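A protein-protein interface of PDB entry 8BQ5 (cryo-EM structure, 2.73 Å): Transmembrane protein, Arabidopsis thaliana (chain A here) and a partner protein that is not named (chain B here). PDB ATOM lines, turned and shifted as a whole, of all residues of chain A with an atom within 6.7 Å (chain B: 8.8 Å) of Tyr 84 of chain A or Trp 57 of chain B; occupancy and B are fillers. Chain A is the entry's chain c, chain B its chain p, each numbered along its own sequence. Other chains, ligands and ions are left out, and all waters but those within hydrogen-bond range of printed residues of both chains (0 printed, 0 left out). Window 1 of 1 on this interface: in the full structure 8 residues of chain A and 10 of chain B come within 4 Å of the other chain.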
ATOM      1  N   GLN A  60      -4.365  27.023 -23.380  1.00  0.00           N
ATOM      2  CA  GLN A  60      -5.593  27.284 -22.637  1.00  0.00           C
ATOM      3  C   GLN A  60      -5.753  26.202 -21.580  1.00  0.00           C
ATOM      4  O   GLN A  60      -5.887  25.022 -21.919  1.00  0.00           O
ATOM      5  CB  GLN A  60      -6.816  27.300 -23.561  1.00  0.00           C
ATOM      6  CG  GLN A  60      -6.682  28.137 -24.834  1.00  0.00           C
ATOM      7  CD  GLN A  60      -6.428  29.608 -24.573  1.00  0.00           C
ATOM      8  OE1 GLN A  60      -7.008  30.201 -23.666  1.00  0.00           O
ATOM      9  NE2 GLN A  60      -5.566  30.211 -25.388  1.00  0.00           N
ATOM     10  N   ARG A  61      -5.749  26.597 -20.305  1.00  0.00           N
ATOM     11  CA  ARG A  61      -5.891  25.666 -19.184  1.00  0.00           C
ATOM     12  C   ARG A  61      -7.196  25.968 -18.460  1.00  0.00           C
ATOM     13  O   ARG A  61      -7.273  26.925 -17.673  1.00  0.00           O
ATOM     14  CB  ARG A  61      -4.704  25.766 -18.228  1.00  0.00           C
ATOM     15  CG  ARG A  61      -3.365  25.977 -18.908  1.00  0.00           C
ATOM     16  CD  ARG A  61      -3.023  24.828 -19.839  1.00  0.00           C
ATOM     17  NE  ARG A  61      -2.591  23.637 -19.117  1.00  0.00           N
ATOM     18  CZ  ARG A  61      -1.378  23.467 -18.612  1.00  0.00           C
ATOM     19  NH1 ARG A  61      -0.449  24.404 -18.712  1.00  0.00           N
ATOM     20  NH2 ARG A  61      -1.088  22.327 -17.993  1.00  0.00           N
ATOM     21  N   PRO A  62      -8.251  25.184 -18.696  1.00  0.00           N
ATOM     22  CA  PRO A  62      -9.540  25.476 -18.047  1.00  0.00           C
ATOM     23  C   PRO A  62      -9.530  25.279 -16.543  1.00  0.00           C
ATOM     24  O   PRO A  62     -10.331  25.916 -15.848  1.00  0.00           O
ATOM     25  CB  PRO A  62     -10.502  24.492 -18.731  1.00  0.00           C
ATOM     26  CG  PRO A  62      -9.798  24.100 -20.000  1.00  0.00           C
ATOM     27  CD  PRO A  62      -8.364  24.023 -19.591  1.00  0.00           C
ATOM     28  N   LYS A  81     -12.254  29.768 -19.152  1.00  0.00           N
ATOM     29  CA  LYS A  81     -13.315  29.248 -20.005  1.00  0.00           C
ATOM     30  C   LYS A  81     -14.542  28.802 -19.213  1.00  0.00           C
ATOM     31  O   LYS A  81     -15.288  27.935 -19.679  1.00  0.00           O
ATOM     32  CB  LYS A  81     -12.781  28.091 -20.850  1.00  0.00           C
ATOM     33  CG  LYS A  81     -11.793  28.515 -21.923  1.00  0.00           C
ATOM     34  CD  LYS A  81     -12.505  29.034 -23.158  1.00  0.00           C
ATOM     35  CE  LYS A  81     -11.644  30.032 -23.912  1.00  0.00           C
ATOM     36  NZ  LYS A  81     -10.192  29.725 -23.792  1.00  0.00           N
ATOM     37  N   ASP A  82     -14.772  29.384 -18.035  1.00  0.00           N
ATOM     38  CA  ASP A  82     -15.859  28.921 -17.177  1.00  0.00           C
ATOM     39  C   ASP A  82     -17.223  29.285 -17.747  1.00  0.00           C
ATOM     40  O   ASP A  82     -18.180  28.509 -17.631  1.00  0.00           O
ATOM     41  CB  ASP A  82     -15.691  29.495 -15.775  1.00  0.00           C
ATOM     42  CG  ASP A  82     -14.463  28.961 -15.083  1.00  0.00           C
ATOM     43  OD1 ASP A  82     -14.154  27.766 -15.273  1.00  0.00           O
ATOM     44  OD2 ASP A  82     -13.803  29.732 -14.357  1.00  0.00           O
ATOM     45  N   ASP A  83     -17.340  30.466 -18.352  1.00  0.00           N
ATOM     46  CA  ASP A  83     -18.593  30.894 -18.974  1.00  0.00           C
ATOM     47  C   ASP A  83     -18.620  30.420 -20.427  1.00  0.00           C
ATOM     48  O   ASP A  83     -18.420  31.182 -21.376  1.00  0.00           O
ATOM     49  CB  ASP A  83     -18.750  32.406 -18.874  1.00  0.00           C
ATOM     50  CG  ASP A  83     -19.132  32.861 -17.483  1.00  0.00           C
ATOM     51  OD1 ASP A  83     -18.566  32.327 -16.507  1.00  0.00           O
ATOM     52  OD2 ASP A  83     -19.999  33.753 -17.365  1.00  0.00           O
ATOM     53  N   TYR A  84     -18.878  29.121 -20.592  1.00  0.00           N
ATOM     54  CA  TYR A  84     -18.875  28.554 -21.933  1.00  0.00           C
ATOM     55  C   TYR A  84     -20.191  28.769 -22.667  1.00  0.00           C
ATOM     56  O   TYR A  84     -20.284  28.410 -23.846  1.00  0.00           O
ATOM     57  CB  TYR A  84     -18.517  27.064 -21.883  1.00  0.00           C
ATOM     58  CG  TYR A  84     -19.275  26.238 -20.869  1.00  0.00           C
ATOM     59  CD1 TYR A  84     -20.628  25.971 -21.026  1.00  0.00           C
ATOM     60  CD2 TYR A  84     -18.634  25.728 -19.750  1.00  0.00           C
ATOM     61  CE1 TYR A  84     -21.315  25.210 -20.102  1.00  0.00           C
ATOM     62  CE2 TYR A  84     -19.315  24.973 -18.819  1.00  0.00           C
ATOM     63  CZ  TYR A  84     -20.656  24.718 -18.999  1.00  0.00           C
ATOM     64  OH  TYR A  84     -21.342  23.965 -18.075  1.00  0.00           O
ATOM     65  N   GLU A  85     -21.202  29.347 -22.013  1.00  0.00           N
ATOM     66  CA  GLU A  85     -22.392  29.771 -22.744  1.00  0.00           C
ATOM     67  C   GLU A  85     -22.098  30.971 -23.633  1.00  0.00           C
ATOM     68  O   GLU A  85     -22.844  31.237 -24.582  1.00  0.00           O
ATOM     69  CB  GLU A  85     -23.529  30.109 -21.777  1.00  0.00           C
ATOM     70  CG  GLU A  85     -23.479  29.404 -20.433  1.00  0.00           C
ATOM     71  CD  GLU A  85     -24.011  27.987 -20.492  1.00  0.00           C
ATOM     72  OE1 GLU A  85     -24.946  27.728 -21.278  1.00  0.00           O
ATOM     73  OE2 GLU A  85     -23.511  27.136 -19.729  1.00  0.00           O
ATOM     74  N   LYS A  86     -21.027  31.709 -23.340  1.00  0.00           N
ATOM     75  CA  LYS A  86     -20.641  32.881 -24.114  1.00  0.00           C
ATOM     76  C   LYS A  86     -19.659  32.565 -25.235  1.00  0.00           C
ATOM     77  O   LYS A  86     -19.232  33.487 -25.937  1.00  0.00           O
ATOM     78  CB  LYS A  86     -20.029  33.946 -23.197  1.00  0.00           C
ATOM     79  CG  LYS A  86     -21.033  34.878 -22.538  1.00  0.00           C
ATOM     80  CD  LYS A  86     -20.397  36.228 -22.219  1.00  0.00           C
ATOM     81  CE  LYS A  86     -19.563  36.172 -20.948  1.00  0.00           C
ATOM     82  NZ  LYS A  86     -20.282  35.497 -19.833  1.00  0.00           N
ATOM     83  N   GLU A  87     -19.280  31.302 -25.413  1.00  0.00           N
ATOM     84  CA  GLU A  87     -18.326  30.958 -26.457  1.00  0.00           C
ATOM     85  C   GLU A  87     -18.967  31.098 -27.831  1.00  0.00           C
ATOM     86  O   GLU A  87     -20.141  30.772 -28.025  1.00  0.00           O
ATOM     87  CB  GLU A  87     -17.804  29.537 -26.252  1.00  0.00           C
ATOM     88  CG  GLU A  87     -16.672  29.447 -25.244  1.00  0.00           C
ATOM     89  CD  GLU A  87     -15.371  30.004 -25.783  1.00  0.00           C
ATOM     90  OE1 GLU A  87     -15.115  29.851 -26.994  1.00  0.00           O
ATOM     91  OE2 GLU A  87     -14.606  30.602 -24.997  1.00  0.00           O
ATOM     92  N   HIS A  88     -18.187  31.586 -28.789  1.00  0.00           N
ATOM     93  CA  HIS A  88     -18.723  31.902 -30.104  1.00  0.00           C
ATOM     94  C   HIS A  88     -17.724  31.608 -31.220  1.00  0.00           C
ATOM     95  O   HIS A  88     -16.640  31.084 -30.973  1.00  0.00           O
ATOM     96  CB  HIS A  88     -19.147  33.367 -30.151  1.00  0.00           C
ATOM     97  CG  HIS A  88     -18.002  34.331 -30.204  1.00  0.00           C
ATOM     98  ND1 HIS A  88     -17.444  34.759 -31.390  1.00  0.00           N
ATOM     99  CD2 HIS A  88     -17.307  34.945 -29.218  1.00  0.00           C
ATOM    100  CE1 HIS A  88     -16.457  35.597 -31.131  1.00  0.00           C
ATOM    101  NE2 HIS A  88     -16.353  35.728 -29.821  1.00  0.00           N
ATOM    102  N   ILE B  50     -21.277  28.197 -33.791  1.00  0.00           N
ATOM    103  CA  ILE B  50     -21.129  28.836 -32.486  1.00  0.00           C
ATOM    104  C   ILE B  50     -21.669  27.925 -31.391  1.00  0.00           C
ATOM    105  O   ILE B  50     -21.081  27.803 -30.310  1.00  0.00           O
ATOM    106  CB  ILE B  50     -21.821  30.211 -32.486  1.00  0.00           C
ATOM    107  CG1 ILE B  50     -20.979  31.214 -33.274  1.00  0.00           C
ATOM    108  CG2 ILE B  50     -22.043  30.708 -31.071  1.00  0.00           C
ATOM    109  CD1 ILE B  50     -21.772  32.332 -33.888  1.00  0.00           C
ATOM    110  N   LEU B  51     -22.794  27.260 -31.663  1.00  0.00           N
ATOM    111  CA  LEU B  51     -23.324  26.278 -30.724  1.00  0.00           C
ATOM    112  C   LEU B  51     -22.382  25.092 -30.562  1.00  0.00           C
ATOM    113  O   LEU B  51     -22.373  24.445 -29.509  1.00  0.00           O
ATOM    114  CB  LEU B  51     -24.701  25.803 -31.191  1.00  0.00           C
ATOM    115  CG  LEU B  51     -25.875  26.762 -30.978  1.00  0.00           C
ATOM    116  CD1 LEU B  51     -27.165  26.156 -31.500  1.00  0.00           C
ATOM    117  CD2 LEU B  51     -26.017  27.131 -29.512  1.00  0.00           C
ATOM    118  N   ARG B  52     -21.592  24.783 -31.594  1.00  0.00           N
ATOM    119  CA  ARG B  52     -20.619  23.700 -31.486  1.00  0.00           C
ATOM    120  C   ARG B  52     -19.482  24.076 -30.546  1.00  0.00           C
ATOM    121  O   ARG B  52     -18.954  23.224 -29.821  1.00  0.00           O
ATOM    122  CB  ARG B  52     -20.080  23.345 -32.872  1.00  0.00           C
ATOM    123  CG  ARG B  52     -18.982  22.296 -32.874  1.00  0.00           C
ATOM    124  CD  ARG B  52     -18.741  21.770 -34.276  1.00  0.00           C
ATOM    125  NE  ARG B  52     -18.177  22.798 -35.142  1.00  0.00           N
ATOM    126  CZ  ARG B  52     -18.180  22.745 -36.467  1.00  0.00           C
ATOM    127  NH1 ARG B  52     -18.694  21.715 -37.117  1.00  0.00           N
ATOM    128  NH2 ARG B  52     -17.652  23.752 -37.156  1.00  0.00           N
ATOM    129  N   GLU B  53     -19.089  25.351 -30.548  1.00  0.00           N
ATOM    130  CA  GLU B  53     -18.017  25.805 -29.668  1.00  0.00           C
ATOM    131  C   GLU B  53     -18.423  25.724 -28.201  1.00  0.00           C
ATOM    132  O   GLU B  53     -17.600  25.392 -27.342  1.00  0.00           O
ATOM    133  CB  GLU B  53     -17.607  27.231 -30.037  1.00  0.00           C
ATOM    134  CG  GLU B  53     -16.180  27.584 -29.648  1.00  0.00           C
ATOM    135  CD  GLU B  53     -15.171  27.239 -30.726  1.00  0.00           C
ATOM    136  OE1 GLU B  53     -14.281  26.405 -30.460  1.00  0.00           O
ATOM    137  OE2 GLU B  53     -15.258  27.808 -31.836  1.00  0.00           O
ATOM    138  N   LYS B  54     -19.687  26.029 -27.895  1.00  0.00           N
ATOM    139  CA  LYS B  54     -20.160  25.930 -26.516  1.00  0.00           C
ATOM    140  C   LYS B  54     -20.080  24.494 -26.012  1.00  0.00           C
ATOM    141  O   LYS B  54     -19.633  24.240 -24.888  1.00  0.00           O
ATOM    142  CB  LYS B  54     -21.593  26.451 -26.407  1.00  0.00           C
ATOM    143  CG  LYS B  54     -21.765  27.929 -26.717  1.00  0.00           C
ATOM    144  CD  LYS B  54     -23.122  28.424 -26.230  1.00  0.00           C
ATOM    145  CE  LYS B  54     -23.689  29.504 -27.134  1.00  0.00           C
ATOM    146  NZ  LYS B  54     -23.430  29.223 -28.567  1.00  0.00           N
ATOM    147  N   VAL B  55     -20.509  23.540 -26.840  1.00  0.00           N
ATOM    148  CA  VAL B  55     -20.448  22.128 -26.469  1.00  0.00           C
ATOM    149  C   VAL B  55     -19.006  21.713 -26.214  1.00  0.00           C
ATOM    150  O   VAL B  55     -18.703  21.000 -25.251  1.00  0.00           O
ATOM    151  CB  VAL B  55     -21.094  21.262 -27.567  1.00  0.00           C
ATOM    152  CG1 VAL B  55     -20.815  19.791 -27.322  1.00  0.00           C
ATOM    153  CG2 VAL B  55     -22.584  21.529 -27.652  1.00  0.00           C
ATOM    154  N   LYS B  56     -18.097  22.162 -27.081  1.00  0.00           N
ATOM    155  CA  LYS B  56     -16.685  21.813 -26.976  1.00  0.00           C
ATOM    156  C   LYS B  56     -16.112  22.209 -25.621  1.00  0.00           C
ATOM    157  O   LYS B  56     -15.473  21.403 -24.937  1.00  0.00           O
ATOM    158  CB  LYS B  56     -15.913  22.495 -28.107  1.00  0.00           C
ATOM    159  CG  LYS B  56     -14.428  22.196 -28.142  1.00  0.00           C
ATOM    160  CD  LYS B  56     -13.705  23.159 -29.076  1.00  0.00           C
ATOM    161  CE  LYS B  56     -14.000  22.851 -30.537  1.00  0.00           C
ATOM    162  NZ  LYS B  56     -15.083  23.707 -31.095  1.00  0.00           N
ATOM    163  N   TRP B  57     -16.336  23.460 -25.217  1.00  0.00           N
ATOM    164  CA  TRP B  57     -15.738  23.944 -23.978  1.00  0.00           C
ATOM    165  C   TRP B  57     -16.531  23.486 -22.760  1.00  0.00           C
ATOM    166  O   TRP B  57     -15.984  23.407 -21.655  1.00  0.00           O
ATOM    167  CB  TRP B  57     -15.611  25.463 -24.022  1.00  0.00           C
ATOM    168  CG  TRP B  57     -14.446  25.910 -24.850  1.00  0.00           C
ATOM    169  CD1 TRP B  57     -14.491  26.561 -26.048  1.00  0.00           C
ATOM    170  CD2 TRP B  57     -13.058  25.732 -24.542  1.00  0.00           C
ATOM    171  NE1 TRP B  57     -13.219  26.801 -26.504  1.00  0.00           N
ATOM    172  CE2 TRP B  57     -12.321  26.302 -25.599  1.00  0.00           C
ATOM    173  CE3 TRP B  57     -12.368  25.147 -23.476  1.00  0.00           C
ATOM    174  CZ2 TRP B  57     -10.929  26.305 -25.619  1.00  0.00           C
ATOM    175  CZ3 TRP B  57     -10.988  25.151 -23.500  1.00  0.00           C
ATOM    176  CH2 TRP B  57     -10.282  25.726 -24.564  1.00  0.00           C
ATOM    177  N   CYS B  58     -17.817  23.180 -22.938  1.00  0.00           N
ATOM    178  CA  CYS B  58     -18.567  22.521 -21.873  1.00  0.00           C
ATOM    179  C   CYS B  58     -17.960  21.162 -21.547  1.00  0.00           C
ATOM    180  O   CYS B  58     -17.712  20.841 -20.379  1.00  0.00           O
ATOM    181  CB  CYS B  58     -20.035  22.376 -22.272  1.00  0.00           C
ATOM    182  SG  CYS B  58     -21.128  21.817 -20.944  1.00  0.00           S
ATOM    183  N   TYR B  59     -17.692  20.358 -22.578  1.00  0.00           N
ATOM    184  CA  TYR B  59     -17.048  19.064 -22.387  1.00  0.00           C
ATOM    185  C   TYR B  59     -15.689  19.224 -21.716  1.00  0.00           C
ATOM    186  O   TYR B  59     -15.306  18.429 -20.849  1.00  0.00           O
ATOM    187  CB  TYR B  59     -16.904  18.356 -23.739  1.00  0.00           C
ATOM    188  CG  TYR B  59     -16.359  16.947 -23.663  1.00  0.00           C
ATOM    189  CD1 TYR B  59     -17.206  15.863 -23.494  1.00  0.00           C
ATOM    190  CD2 TYR B  59     -14.996  16.702 -23.769  1.00  0.00           C
ATOM    191  CE1 TYR B  59     -16.716  14.580 -23.430  1.00  0.00           C
ATOM    192  CE2 TYR B  59     -14.496  15.419 -23.704  1.00  0.00           C
ATOM    193  CZ  TYR B  59     -15.362  14.361 -23.534  1.00  0.00           C
ATOM    194  OH  TYR B  59     -14.879  13.079 -23.467  1.00  0.00           O
ATOM    195  N   ARG B  60     -14.944  20.251 -22.123  1.00  0.00           N
ATOM    196  CA  ARG B  60     -13.559  20.433 -21.606  1.00  0.00           C
ATOM    197  C   ARG B  60     -13.575  20.949 -20.163  1.00  0.00           C
ATOM    198  O   ARG B  60     -12.686  20.547 -19.397  1.00  0.00           O
ATOM    199  CB  ARG B  60     -12.790  21.378 -22.530  1.00  0.00           C
ATOM    200  CG  ARG B  60     -12.522  20.784 -23.905  1.00  0.00           C
ATOM    201  CD  ARG B  60     -11.910  21.767 -24.878  1.00  0.00           C
ATOM    202  NE  ARG B  60     -11.570  21.111 -26.131  1.00  0.00           N
ATOM    203  CZ  ARG B  60     -10.909  21.688 -27.124  1.00  0.00           C
ATOM    204  NH1 ARG B  60     -10.506  22.941 -27.009  1.00  0.00           N
ATOM    205  NH2 ARG B  60     -10.647  21.010 -28.226  1.00  0.00           N
ATOM    206  N   VAL B  61     -14.528  21.816 -19.819  1.00  0.00           N
ATOM    207  CA  VAL B  61     -14.554  22.391 -18.478  1.00  0.00           C
ATOM    208  C   VAL B  61     -15.110  21.397 -17.464  1.00  0.00           C
ATOM    209  O   VAL B  61     -14.564  21.245 -16.366  1.00  0.00           O
ATOM    210  CB  VAL B  61     -15.354  23.707 -18.484  1.00  0.00           C
ATOM    211  CG1 VAL B  61     -15.878  24.032 -17.093  1.00  0.00           C
ATOM    212  CG2 VAL B  61     -14.497  24.844 -19.011  1.00  0.00           C
ATOM    213  N   GLU B  62     -16.187  20.699 -17.815  1.00  0.00           N
ATOM    214  CA  GLU B  62     -16.937  19.905 -16.851  1.00  0.00           C
ATOM    215  C   GLU B  62     -16.402  18.491 -16.663  1.00  0.00           C
ATOM    216  O   GLU B  62     -16.788  17.831 -15.693  1.00  0.00           O
ATOM    217  CB  GLU B  62     -18.408  19.843 -17.267  1.00  0.00           C
ATOM    218  CG  GLU B  62     -19.037  21.210 -17.480  1.00  0.00           C
ATOM    219  CD  GLU B  62     -19.316  21.937 -16.179  1.00  0.00           C
ATOM    220  OE1 GLU B  62     -19.638  23.143 -16.230  1.00  0.00           O
ATOM    221  OE2 GLU B  62     -19.224  21.304 -15.107  1.00  0.00           O
ATOM    222  N   GLY B  63     -15.528  18.015 -17.547  1.00  0.00           N
ATOM    223  CA  GLY B  63     -14.952  16.691 -17.375  1.00  0.00           C
ATOM    224  C   GLY B  63     -16.004  15.599 -17.354  1.00  0.00           C
ATOM    225  O   GLY B  63     -16.898  15.542 -18.204  1.00  0.00           O
ATOM    226  N   ASN B  65     -18.419  15.278 -15.587  1.00  0.00           N
ATOM    227  CA  ASN B  65     -19.783  15.783 -15.283  1.00  0.00           C
ATOM    228  C   ASN B  65     -20.434  16.394 -16.530  1.00  0.00           C
ATOM    229  O   ASN B  65     -21.440  17.088 -16.356  1.00  0.00           O
ATOM    230  CB  ASN B  65     -19.745  16.766 -14.109  1.00  0.00           C
ATOM    231  CG  ASN B  65     -19.048  16.189 -12.898  1.00  0.00           C
ATOM    232  OD1 ASN B  65     -19.386  15.101 -12.444  1.00  0.00           O
ATOM    233  ND2 ASN B  65     -18.065  16.906 -12.382  1.00  0.00           N
ATOM    234  N   HIS B  66     -19.910  16.088 -17.712  1.00  0.00           N
ATOM    235  CA  HIS B  66     -20.418  16.718 -18.960  1.00  0.00           C
ATOM    236  C   HIS B  66     -21.801  16.182 -19.336  1.00  0.00           C
ATOM    237  O   HIS B  66     -22.599  16.970 -19.827  1.00  0.00           O
ATOM    238  CB  HIS B  66     -19.381  16.540 -20.072  1.00  0.00           C
ATOM    239  CG  HIS B  66     -19.368  15.194 -20.710  1.00  0.00           C
ATOM    240  ND1 HIS B  66     -20.096  14.915 -21.847  1.00  0.00           N
ATOM    241  CD2 HIS B  66     -18.716  14.057 -20.387  1.00  0.00           C
ATOM    242  CE1 HIS B  66     -19.895  13.664 -22.194  1.00  0.00           C
ATOM    243  NE2 HIS B  66     -19.052  13.115 -21.315  1.00  0.00           N
ATOM    244  N   GLN B  68     -24.396  15.320 -17.567  1.00  0.00           N
ATOM    245  CA  GLN B  68     -25.467  15.988 -16.791  1.00  0.00           C
ATOM    246  C   GLN B  68     -25.413  17.501 -17.009  1.00  0.00           C
ATOM    247  O   GLN B  68     -26.492  18.113 -17.029  1.00  0.00           O
ATOM    248  CB  GLN B  68     -25.283  15.592 -15.323  1.00  0.00           C
ATOM    249  CG  GLN B  68     -26.365  16.055 -14.361  1.00  0.00           C
ATOM    250  CD  GLN B  68     -26.146  15.454 -12.996  1.00  0.00           C
ATOM    251  OE1 GLN B  68     -25.255  14.632 -12.793  1.00  0.00           O
ATOM    252  NE2 GLN B  68     -26.981  15.850 -12.049  1.00  0.00           N
ATOM    253  N   LYS B  69     -24.226  18.071 -17.243  1.00  0.00           N
ATOM    254  CA  LYS B  69     -24.091  19.554 -17.316  1.00  0.00           C
ATOM    255  C   LYS B  69     -24.277  20.100 -18.735  1.00  0.00           C
ATOM    256  O   LYS B  69     -24.855  21.196 -18.855  1.00  0.00           O
ATOM    257  CB  LYS B  69     -22.733  19.984 -16.758  1.00  0.00           C
ATOM    258  CG  LYS B  69     -22.779  20.598 -15.368  1.00  0.00           C
ATOM    259  CD  LYS B  69     -22.668  19.572 -14.263  1.00  0.00           C
ATOM    260  CE  LYS B  69     -22.374  20.182 -12.911  1.00  0.00           C
ATOM    261  NZ  LYS B  69     -21.594  19.261 -12.049  1.00  0.00           N
ATOM    262  N   CYS B  70     -23.806  19.389 -19.762  1.00  0.00           N
ATOM    263  CA  CYS B  70     -23.884  19.889 -21.160  1.00  0.00           C
ATOM    264  C   CYS B  70     -25.114  19.335 -21.874  1.00  0.00           C
ATOM    265  O   CYS B  70     -25.251  19.611 -23.074  1.00  0.00           O
ATOM    266  CB  CYS B  70     -22.661  19.441 -21.947  1.00  0.00           C
ATOM    267  SG  CYS B  70     -21.108  19.800 -21.094  1.00  0.00           S
ATOM    268  N   ARG B  71     -25.959  18.573 -21.174  1.00  0.00           N
ATOM    269  CA  ARG B  71     -27.169  17.949 -21.777  1.00  0.00           C
ATOM    270  C   ARG B  71     -27.911  18.942 -22.678  1.00  0.00           C
ATOM    271  O   ARG B  71     -28.241  18.562 -23.819  1.00  0.00           O
ATOM    272  CB  ARG B  71     -28.100  17.492 -20.652  1.00  0.00           C
ATOM    273  CG  ARG B  71     -28.778  16.152 -20.894  1.00  0.00           C
ATOM    274  CD  ARG B  71     -30.030  16.025 -20.049  1.00  0.00           C
ATOM    275  NE  ARG B  71     -31.188  16.596 -20.722  1.00  0.00           N
ATOM    276  CZ  ARG B  71     -32.081  15.903 -21.420  1.00  0.00           C
ATOM    277  NH1 ARG B  71     -31.964  14.592 -21.541  1.00  0.00           N
ATOM    278  NH2 ARG B  71     -33.091  16.528 -21.995  1.00  0.00           N
ATOM    279  N   HIS B  72     -28.159  20.158 -22.188  1.00  0.00           N
ATOM    280  CA  HIS B  72     -28.931  21.184 -22.938  1.00  0.00           C
ATOM    281  C   HIS B  72     -28.161  21.659 -24.177  1.00  0.00           C
ATOM    282  O   HIS B  72     -28.791  21.754 -25.237  1.00  0.00           O
ATOM    283  CB  HIS B  72     -29.295  22.347 -21.995  1.00  0.00           C
ATOM    284  CG  HIS B  72     -28.129  23.155 -21.529  1.00  0.00           C
ATOM    285  ND1 HIS B  72     -27.980  24.488 -21.860  1.00  0.00           N
ATOM    286  CD2 HIS B  72     -27.051  22.829 -20.783  1.00  0.00           C
ATOM    287  CE1 HIS B  72     -26.869  24.950 -21.324  1.00  0.00           C
ATOM    288  NE2 HIS B  72     -26.276  23.951 -20.665  1.00  0.00           N
ATOM    289  N   LEU B  73     -26.866  21.957 -24.042  1.00  0.00           N
ATOM    290  CA  LEU B  73     -26.051  22.480 -25.169  1.00  0.00           C
ATOM    291  C   LEU B  73     -25.969  21.415 -26.265  1.00  0.00           C
ATOM    292  O   LEU B  73     -26.050  21.797 -27.445  1.00  0.00           O
ATOM    293  CB  LEU B  73     -24.662  22.844 -24.636  1.00  0.00           C
ATOM    294  CG  LEU B  73     -24.575  24.189 -23.922  1.00  0.00           C
ATOM    295  CD1 LEU B  73     -23.161  24.460 -23.442  1.00  0.00           C
ATOM    296  CD2 LEU B  73     -25.063  25.314 -24.818  1.00  0.00           C
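Of the 11 printed residues of chain A, 7 touch a printed residue of chain B. Hydrophobic or aromatic side chains of chain A within 4 Å of the printed part of chain B: Pro 62 and Tyr 84. Of the 22 printed residues of chain B, 9 touch a printed residue of chain A. Hydrophobic or aromatic side chains of chain B that line the printed part of chain A: Ile 50, Trp 57, Val 61, His 72 and Leu 73. Among the printed residues, 18 pairs touch across the chains. Among the printed residues, no Asp or Glu carboxylate lies within 4 Å of a Lys or Arg side-chain nitrogen of the other chain.
The side-chain sulfur (SG) of Cys 58 of chain B sits close to the side-chain hydroxyl (OH) of Tyr 84 of chain A (3.6 Å). OE1 of Glu 62 of chain B lies within hydrogen-bond range of OH of Tyr 84 of chain A (2.6 Å).
Of chain B, only Lys 54 (3.3 Å), Trp 57 (3.9 Å), Cys 58 (3.5 Å), Val 61 (3.96 Å), Glu 62 (2.6 Å) and Leu 73 (3.8 Å) come within 4 Å of Tyr 84 of chain A. Printed residues of chain A within 4 Å of Trp 57 of chain B: Gln 60 (3.9 Å), Pro 62 (3.8 Å), Lys 81 (3.6 Å), Tyr 84 (3.9 Å) and Glu 87 (3.5 Å). Of chain B, only Lys 54 and His 72 come within 4 Å of Glu 85 of chain A. Of the printed residues of chain A, Val 61 of chain B touches Lys 81 and Tyr 84. Printed residues of chain A within 4 Å of Leu 73 of chain B: Tyr 84 (3.8 Å). Asn 65 of chain B touches none of the printed residues of chain A. The nearest residue of chain A that does not touch Trp 57 of chain B is Arg 61 of chain A (6.3 Å). The nearest printed residue of chain A that does not touch Lys 54 of chain B is Lys 86 of chain A (4.9 Å).
OE1 of Gln 60 of chain A is in hydrogen-bond range of NZ of Lys 81 of chain A (3.2 Å). The backbone carbonyl oxygen of Ile 50 of chain B lies close to the side-chain amino group of Lys 54 of chain B. The side-chain amino group (NZ) of Lys 56 of chain B is in salt-bridge range of the side-chain carboxylate (OE1) of Glu 53 of chain B (2.9 Å). SG of Cys 58 of chain B is disulfide-bonded to SG of Cys 70 of chain B (2.0 Å).
Among the printed residues, merely in contact across the chains: Glu 85 of chain A with Lys 54 of chain B (3.2 Å), Lys 81 of chain A with Val 61 of chain B (3.3 Å), Tyr 84 of chain A with Lys 54 of chain B (3.3 Å), Glu 85 of chain A with His 72 of chain B (3.4 Å), Glu 87 of chain A with Trp 57 of chain B (3.5 Å), Glu 87 of chain A with Lys 54 of chain B (3.5 Å), Glu 87 of chain A with Ile 50 of chain B (3.6 Å), Lys 81 of chain A with Trp 57 of chain B (3.6 Å), Glu 87 of chain A with Glu 53 of chain B (3.6 Å), His 88 of chain A with Ile 50 of chain B (3.7 Å), His 88 of chain A with Glu 53 of chain B (3.7 Å), Tyr 84 of chain A with Leu 73 of chain B (3.8 Å), Pro 62 of chain A with Trp 57 of chain B (3.8 Å), Gln 60 of chain A with Trp 57 of chain B (3.9 Å), Tyr 84 of chain A with Trp 57 of chain B (3.9 Å) and Tyr 84 of chain A with Val 61 of chain B (3.96 Å).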
